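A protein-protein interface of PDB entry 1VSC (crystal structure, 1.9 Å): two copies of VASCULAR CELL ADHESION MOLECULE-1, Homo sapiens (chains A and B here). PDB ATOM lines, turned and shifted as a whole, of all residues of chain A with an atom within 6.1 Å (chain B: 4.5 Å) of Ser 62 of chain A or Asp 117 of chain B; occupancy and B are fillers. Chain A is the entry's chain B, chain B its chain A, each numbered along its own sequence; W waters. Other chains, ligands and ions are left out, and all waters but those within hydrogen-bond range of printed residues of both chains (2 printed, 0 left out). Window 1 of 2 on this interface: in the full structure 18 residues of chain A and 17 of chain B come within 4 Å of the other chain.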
ATOM      1  N   ILE A  15      -6.490  -4.741 -21.530  1.00  0.00           N
ATOM      2  CA  ILE A  15      -5.608  -3.676 -21.996  1.00  0.00           C
ATOM      3  C   ILE A  15      -5.614  -2.530 -20.978  1.00  0.00           C
ATOM      4  O   ILE A  15      -6.616  -2.298 -20.324  1.00  0.00           O
ATOM      5  CB  ILE A  15      -6.047  -3.181 -23.336  1.00  0.00           C
ATOM      6  CG1 ILE A  15      -6.013  -4.355 -24.296  1.00  0.00           C
ATOM      7  CG2 ILE A  15      -5.172  -2.001 -23.805  1.00  0.00           C
ATOM      8  CD1 ILE A  15      -5.652  -3.972 -25.684  1.00  0.00           C
ATOM      9  N   GLY A  16      -4.463  -1.917 -20.743  1.00  0.00           N
ATOM     10  CA  GLY A  16      -4.394  -0.848 -19.770  1.00  0.00           C
ATOM     11  C   GLY A  16      -4.169  -1.281 -18.345  1.00  0.00           C
ATOM     12  O   GLY A  16      -4.035  -0.439 -17.441  1.00  0.00           O
ATOM     13  N   ASP A  17      -4.173  -2.578 -18.079  1.00  0.00           N
ATOM     14  CA  ASP A  17      -3.930  -3.028 -16.708  1.00  0.00           C
ATOM     15  C   ASP A  17      -2.428  -2.949 -16.399  1.00  0.00           C
ATOM     16  O   ASP A  17      -1.596  -2.855 -17.285  1.00  0.00           O
ATOM     17  CB  ASP A  17      -4.345  -4.490 -16.550  1.00  0.00           C
ATOM     18  CG  ASP A  17      -5.875  -4.700 -16.421  1.00  0.00           C
ATOM     19  OD1 ASP A  17      -6.648  -3.703 -16.260  1.00  0.00           O
ATOM     20  OD2 ASP A  17      -6.275  -5.907 -16.424  1.00  0.00           O
ATOM     21  N   MET A  58       4.676  -4.623 -16.733  1.00  0.00           N
ATOM     22  CA  MET A  58       4.203  -4.073 -18.000  1.00  0.00           C
ATOM     23  C   MET A  58       3.010  -3.283 -17.569  1.00  0.00           C
ATOM     24  O   MET A  58       1.957  -3.876 -17.295  1.00  0.00           O
ATOM     25  CB  MET A  58       3.756  -5.202 -18.914  1.00  0.00           C
ATOM     26  CG  MET A  58       4.969  -5.974 -19.427  1.00  0.00           C
ATOM     27  SD  MET A  58       4.606  -7.634 -19.930  1.00  0.00           S
ATOM     28  CE  MET A  58       4.262  -8.273 -18.331  1.00  0.00           C
ATOM     29  N   PRO A  60       1.062   0.564 -18.611  1.00  0.00           N
ATOM     30  CA  PRO A  60      -0.147  -0.249 -18.838  1.00  0.00           C
ATOM     31  C   PRO A  60       0.087  -1.387 -19.846  1.00  0.00           C
ATOM     32  O   PRO A  60       0.846  -1.238 -20.798  1.00  0.00           O
ATOM     33  CB  PRO A  60      -1.129   0.810 -19.387  1.00  0.00           C
ATOM     34  CG  PRO A  60      -0.300   1.617 -20.234  1.00  0.00           C
ATOM     35  CD  PRO A  60       0.884   1.878 -19.281  1.00  0.00           C
ATOM     36  N   VAL A  61      -0.470  -2.552 -19.610  1.00  0.00           N
ATOM     37  CA  VAL A  61      -0.248  -3.621 -20.568  1.00  0.00           C
ATOM     38  C   VAL A  61      -0.937  -3.267 -21.908  1.00  0.00           C
ATOM     39  O   VAL A  61      -2.006  -2.626 -21.949  1.00  0.00           O
ATOM     40  CB  VAL A  61      -0.716  -4.989 -20.016  1.00  0.00           C
ATOM     41  CG1 VAL A  61      -2.272  -5.089 -19.927  1.00  0.00           C
ATOM     42  CG2 VAL A  61      -0.104  -6.105 -20.854  1.00  0.00           C
ATOM     43  N   SER A  62      -0.335  -3.671 -23.014  1.00  0.00           N
ATOM     44  CA  SER A  62      -0.860  -3.341 -24.300  1.00  0.00           C
ATOM     45  C   SER A  62      -0.492  -4.421 -25.283  1.00  0.00           C
ATOM     46  O   SER A  62       0.037  -5.452 -24.855  1.00  0.00           O
ATOM     47  CB  SER A  62      -0.257  -2.011 -24.705  1.00  0.00           C
ATOM     48  OG  SER A  62      -0.594  -1.686 -26.018  1.00  0.00           O
ATOM     49  N   PHE A  63      -0.699  -4.208 -26.555  1.00  0.00           N
ATOM     50  CA  PHE A  63      -0.440  -5.192 -27.593  1.00  0.00           C
ATOM     51  C   PHE A  63       0.980  -5.618 -27.751  1.00  0.00           C
ATOM     52  O   PHE A  63       1.266  -6.642 -28.325  1.00  0.00           O
ATOM     53  CB  PHE A  63      -0.857  -4.697 -28.980  1.00  0.00           C
ATOM     54  CG  PHE A  63      -2.318  -4.377 -29.024  1.00  0.00           C
ATOM     55  CD1 PHE A  63      -3.251  -5.384 -29.162  1.00  0.00           C
ATOM     56  CD2 PHE A  63      -2.757  -3.061 -28.845  1.00  0.00           C
ATOM     57  CE1 PHE A  63      -4.607  -5.106 -29.080  1.00  0.00           C
ATOM     58  CE2 PHE A  63      -4.119  -2.766 -28.768  1.00  0.00           C
ATOM     59  CZ  PHE A  63      -5.045  -3.793 -28.868  1.00  0.00           C
ATOM     60  N   GLY A  64       1.898  -4.770 -27.278  1.00  0.00           N
ATOM     61  CA  GLY A  64       3.281  -5.111 -27.421  1.00  0.00           C
ATOM     62  C   GLY A  64       3.723  -6.026 -26.320  1.00  0.00           C
ATOM     63  O   GLY A  64       4.909  -6.348 -26.256  1.00  0.00           O
ATOM     64  N   ASN A  65       2.780  -6.398 -25.460  1.00  0.00           N
ATOM     65  CA  ASN A  65       3.059  -7.283 -24.345  1.00  0.00           C
ATOM     66  C   ASN A  65       2.429  -8.626 -24.585  1.00  0.00           C
ATOM     67  O   ASN A  65       2.412  -9.495 -23.723  1.00  0.00           O
ATOM     68  CB  ASN A  65       2.444  -6.748 -23.106  1.00  0.00           C
ATOM     69  CG  ASN A  65       3.104  -5.528 -22.632  1.00  0.00           C
ATOM     70  OD1 ASN A  65       2.422  -4.600 -22.277  1.00  0.00           O
ATOM     71  ND2 ASN A  65       4.422  -5.501 -22.612  1.00  0.00           N
ATOM     72  N   GLU A  66       1.840  -8.796 -25.743  1.00  0.00           N
ATOM     73  CA  GLU A  66       1.168 -10.046 -26.014  1.00  0.00           C
ATOM     74  C   GLU A  66       2.204 -11.038 -26.530  1.00  0.00           C
ATOM     75  O   GLU A  66       2.489 -11.092 -27.720  1.00  0.00           O
ATOM     76  CB  GLU A  66       0.085  -9.768 -27.036  1.00  0.00           C
ATOM     77  CG  GLU A  66      -0.962 -10.795 -27.084  1.00  0.00           C
ATOM     78  CD  GLU A  66      -2.161 -10.304 -27.842  1.00  0.00           C
ATOM     79  OE1 GLU A  66      -1.990  -9.850 -29.009  1.00  0.00           O
ATOM     80  OE2 GLU A  66      -3.264 -10.385 -27.249  1.00  0.00           O
ATOM     81  N   ILE A  88      -4.270 -10.556 -23.643  1.00  0.00           N
ATOM     82  CA  ILE A  88      -5.062  -9.365 -23.297  1.00  0.00           C
ATOM     83  C   ILE A  88      -6.463  -9.425 -23.874  1.00  0.00           C
ATOM     84  O   ILE A  88      -6.676 -10.076 -24.891  1.00  0.00           O
ATOM     85  CB  ILE A  88      -4.394  -8.017 -23.802  1.00  0.00           C
ATOM     86  CG1 ILE A  88      -3.925  -8.150 -25.232  1.00  0.00           C
ATOM     87  CG2 ILE A  88      -3.255  -7.586 -22.936  1.00  0.00           C
ATOM     88  CD1 ILE A  88      -3.456  -6.793 -25.851  1.00  0.00           C
ATOM     89  N   SER B  90      -0.713   9.228 -27.531  1.00  0.00           N
ATOM     90  CA  SER B  90      -0.386   8.148 -26.592  1.00  0.00           C
ATOM     91  C   SER B  90       1.126   8.194 -26.340  1.00  0.00           C
ATOM     92  O   SER B  90       1.906   8.242 -27.299  1.00  0.00           O
ATOM     93  CB  SER B  90      -0.712   6.822 -27.259  1.00  0.00           C
ATOM     94  OG  SER B  90      -0.778   5.796 -26.298  1.00  0.00           O
ATOM     95  N   PHE B  91       1.525   8.202 -25.073  1.00  0.00           N
ATOM     96  CA  PHE B  91       2.955   8.220 -24.677  1.00  0.00           C
ATOM     97  C   PHE B  91       2.879   7.668 -23.261  1.00  0.00           C
ATOM     98  O   PHE B  91       3.395   8.267 -22.317  1.00  0.00           O
ATOM     99  CB  PHE B  91       3.466   9.662 -24.615  1.00  0.00           C
ATOM    100  CG  PHE B  91       4.975   9.798 -24.661  1.00  0.00           C
ATOM    101  CD1 PHE B  91       5.761   8.853 -25.291  1.00  0.00           C
ATOM    102  CD2 PHE B  91       5.606  10.885 -24.062  1.00  0.00           C
ATOM    103  CE1 PHE B  91       7.175   8.982 -25.312  1.00  0.00           C
ATOM    104  CE2 PHE B  91       7.049  11.027 -24.080  1.00  0.00           C
ATOM    105  CZ  PHE B  91       7.822  10.075 -24.701  1.00  0.00           C
ATOM    106  N   PRO B  92       2.352   6.442 -23.114  1.00  0.00           N
ATOM    107  CA  PRO B  92       2.215   5.870 -21.781  1.00  0.00           C
ATOM    108  C   PRO B  92       3.434   5.186 -21.113  1.00  0.00           C
ATOM    109  O   PRO B  92       3.355   4.876 -19.931  1.00  0.00           O
ATOM    110  CB  PRO B  92       1.105   4.844 -22.001  1.00  0.00           C
ATOM    111  CG  PRO B  92       1.460   4.284 -23.345  1.00  0.00           C
ATOM    112  CD  PRO B  92       2.031   5.438 -24.151  1.00  0.00           C
ATOM    113  N   LYS B  93       4.533   4.978 -21.831  1.00  0.00           N
ATOM    114  CA  LYS B  93       5.666   4.224 -21.237  1.00  0.00           C
ATOM    115  C   LYS B  93       7.077   4.794 -21.452  1.00  0.00           C
ATOM    116  O   LYS B  93       7.385   5.403 -22.508  1.00  0.00           O
ATOM    117  CB  LYS B  93       5.630   2.776 -21.759  1.00  0.00           C
ATOM    118  CG  LYS B  93       4.676   1.850 -21.023  1.00  0.00           C
ATOM    119  CD  LYS B  93       4.415   0.648 -21.906  1.00  0.00           C
ATOM    120  CE  LYS B  93       4.027  -0.590 -21.084  1.00  0.00           C
ATOM    121  NZ  LYS B  93       3.588  -1.775 -21.913  1.00  0.00           N
ATOM    122  N   VAL B 115      10.651   2.530 -27.692  1.00  0.00           N
ATOM    123  CA  VAL B 115       9.494   3.176 -27.017  1.00  0.00           C
ATOM    124  C   VAL B 115       8.243   2.472 -27.502  1.00  0.00           C
ATOM    125  O   VAL B 115       8.055   2.319 -28.702  1.00  0.00           O
ATOM    126  CB  VAL B 115       9.222   4.643 -27.328  1.00  0.00           C
ATOM    127  CG1 VAL B 115       8.933   5.350 -26.035  1.00  0.00           C
ATOM    128  CG2 VAL B 115      10.311   5.267 -28.093  1.00  0.00           C
ATOM    129  N   ALA B 116       7.395   2.071 -26.564  1.00  0.00           N
ATOM    130  CA  ALA B 116       6.154   1.371 -26.866  1.00  0.00           C
ATOM    131  C   ALA B 116       4.925   2.291 -26.785  1.00  0.00           C
ATOM    132  O   ALA B 116       4.969   3.320 -26.071  1.00  0.00           O
ATOM    133  CB  ALA B 116       5.967   0.260 -25.858  1.00  0.00           C
ATOM    134  N   ASP B 117       3.892   1.941 -27.574  1.00  0.00           N
ATOM    135  CA  ASP B 117       2.580   2.579 -27.537  1.00  0.00           C
ATOM    136  C   ASP B 117       2.509   4.067 -27.793  1.00  0.00           C
ATOM    137  O   ASP B 117       1.748   4.779 -27.144  1.00  0.00           O
ATOM    138  CB  ASP B 117       1.940   2.274 -26.181  1.00  0.00           C
ATOM    139  CG  ASP B 117       1.820   0.771 -25.925  1.00  0.00           C
ATOM    140  OD1 ASP B 117       1.673   0.038 -26.930  1.00  0.00           O
ATOM    141  OD2 ASP B 117       1.883   0.323 -24.741  1.00  0.00           O
ATOM    142  N   VAL B 118       3.251   4.514 -28.788  1.00  0.00           N
ATOM    143  CA  VAL B 118       3.313   5.908 -29.098  1.00  0.00           C
ATOM    144  C   VAL B 118       2.412   6.278 -30.264  1.00  0.00           C
ATOM    145  O   VAL B 118       2.318   5.533 -31.268  1.00  0.00           O
ATOM    146  CB  VAL B 118       4.755   6.303 -29.488  1.00  0.00           C
ATOM    147  CG1 VAL B 118       4.753   7.738 -30.083  1.00  0.00           C
ATOM    148  CG2 VAL B 118       5.649   6.263 -28.268  1.00  0.00           C
ATOM    149  N   TYR B 119       1.733   7.415 -30.105  1.00  0.00           N
ATOM    150  CA  TYR B 119       0.915   7.986 -31.177  1.00  0.00           C
ATOM    151  C   TYR B 119       0.789   9.492 -30.975  1.00  0.00           C
ATOM    152  O   TYR B 119       0.574   9.949 -29.840  1.00  0.00           O
ATOM    153  CB  TYR B 119      -0.472   7.354 -31.266  1.00  0.00           C
ATOM    154  CG  TYR B 119      -1.275   7.919 -32.443  1.00  0.00           C
ATOM    155  CD1 TYR B 119      -1.067   7.460 -33.749  1.00  0.00           C
ATOM    156  CD2 TYR B 119      -2.225   8.929 -32.242  1.00  0.00           C
ATOM    157  CE1 TYR B 119      -1.772   7.994 -34.811  1.00  0.00           C
ATOM    158  CE2 TYR B 119      -2.941   9.471 -33.323  1.00  0.00           C
ATOM    159  CZ  TYR B 119      -2.714   8.991 -34.580  1.00  0.00           C
ATOM    160  OH  TYR B 119      -3.457   9.484 -35.610  1.00  0.00           O
ATOM    161  N   LEU B 149       0.378   1.763 -32.892  1.00  0.00           N
ATOM    162  CA  LEU B 149       0.692   1.609 -31.458  1.00  0.00           C
ATOM    163  C   LEU B 149       1.850   0.606 -31.342  1.00  0.00           C
ATOM    164  O   LEU B 149       2.043  -0.028 -30.291  1.00  0.00           O
ATOM    165  CB  LEU B 149      -0.501   1.076 -30.643  1.00  0.00           C
ATOM    166  CG  LEU B 149      -1.308   2.012 -29.757  1.00  0.00           C
ATOM    167  CD1 LEU B 149      -1.849   1.269 -28.555  1.00  0.00           C
ATOM    168  CD2 LEU B 149      -0.459   3.146 -29.317  1.00  0.00           C
ATOM    169  N   GLU B 150       2.632   0.507 -32.416  1.00  0.00           N
ATOM    170  CA  GLU B 150       3.751  -0.402 -32.504  1.00  0.00           C
ATOM    171  C   GLU B 150       4.961   0.261 -31.851  1.00  0.00           C
ATOM    172  O   GLU B 150       5.078   1.484 -31.846  1.00  0.00           O
ATOM    173  CB  GLU B 150       4.046  -0.680 -33.964  1.00  0.00           C
ATOM    174  CG  GLU B 150       4.020  -2.147 -34.329  1.00  0.00           C
ATOM    175  CD  GLU B 150       4.066  -2.372 -35.832  1.00  0.00           C
ATOM    176  OE1 GLU B 150       5.171  -2.227 -36.416  1.00  0.00           O
ATOM    177  OE2 GLU B 150       2.994  -2.663 -36.428  1.00  0.00           O
HETATM  178  O   HOH W   1       0.274  -1.857 -28.468  1.00  0.00           O
HETATM  179  O   HOH W   2       2.256  -2.339 -26.511  1.00  0.00           O
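Ser 62 of chain A touches just one residue of chain B: Asp 117.
Printed residues of chain A within 4 Å of Pro 92 of chain B: Pro 60 (3.9 Å).
Of the printed residues of chain B, Pro 60 of chain A touches Pro 92 (3.9 Å) and Lys 93 (3.0 Å).
Val 61 of chain A touches none of the printed residues of chain B.
Asp 17 of chain A touches none of the printed residues of chain B.
The nearest residue of chain A that does not touch Asp 117 of chain B is Pro 60 of chain A (4.4 Å).
No position is printed for both chains.
Water W2 lies within hydrogen-bond range of OD1 of Asp 117 of chain B (2.5 Å), N of Gly 64 of chain A (2.6 Å), OG of Ser 62 of chain A (3.0 Å) and N of Phe 63 of chain A (3.5 Å).
Water W1 lies within hydrogen-bond range of the side-chain hydroxyl of Ser 62 of chain A, the side-chain carboxylate of Asp 117 of chain B, the backbone carbonyl oxygen of Leu 149 of chain B and the backbone NH of Phe 63 of chain A.
The backbone carbonyl oxygen (O) of Asp 117 of chain B sits at hydrogen-bond distance from the side-chain hydroxyl (OG) of Ser 90 of chain B, at 2.9 Å.
NZ of Lys 93 of chain B is in salt-bridge range of OD2 of Asp 117 of chain B (3.9 Å).
The side-chain amide nitrogen (ND2) of Asn 65 of chain A sits close to the side-chain sulfur (SD) of Met 58 of chain A, at 3.4 Å.
OD1 of Asn 65 of chain A sits at hydrogen-bond distance from N of Ser 62 of chain A (3.0 Å).
Pro 60 of chain A touches Pro 92 of chain B.
The side-chain amino group (NZ) of Lys 93 of chain B is in hydrogen-bond range of the backbone carbonyl oxygen (O) of Pro 60 of chain A, at 3.0 Å.
The side-chain amide oxygen of Asn 65 of chain A is in hydrogen-bond range of the side-chain amino group of Lys 93 of chain B (3.1 Å).
OD1 of Asp 117 of chain B sits at hydrogen-bond distance from OG of Ser 62 of chain A, 3.0 Å away.
Hydrophobic or aromatic side chains of chain B within 4 Å of the printed part of chain A: Pro 92.
Of the 12 printed residues of chain A, 3 touch a printed residue of chain B.
Among the printed residues, no Asp or Glu carboxylate lies within 4 Å of a Lys or Arg side-chain nitrogen of the other chain.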
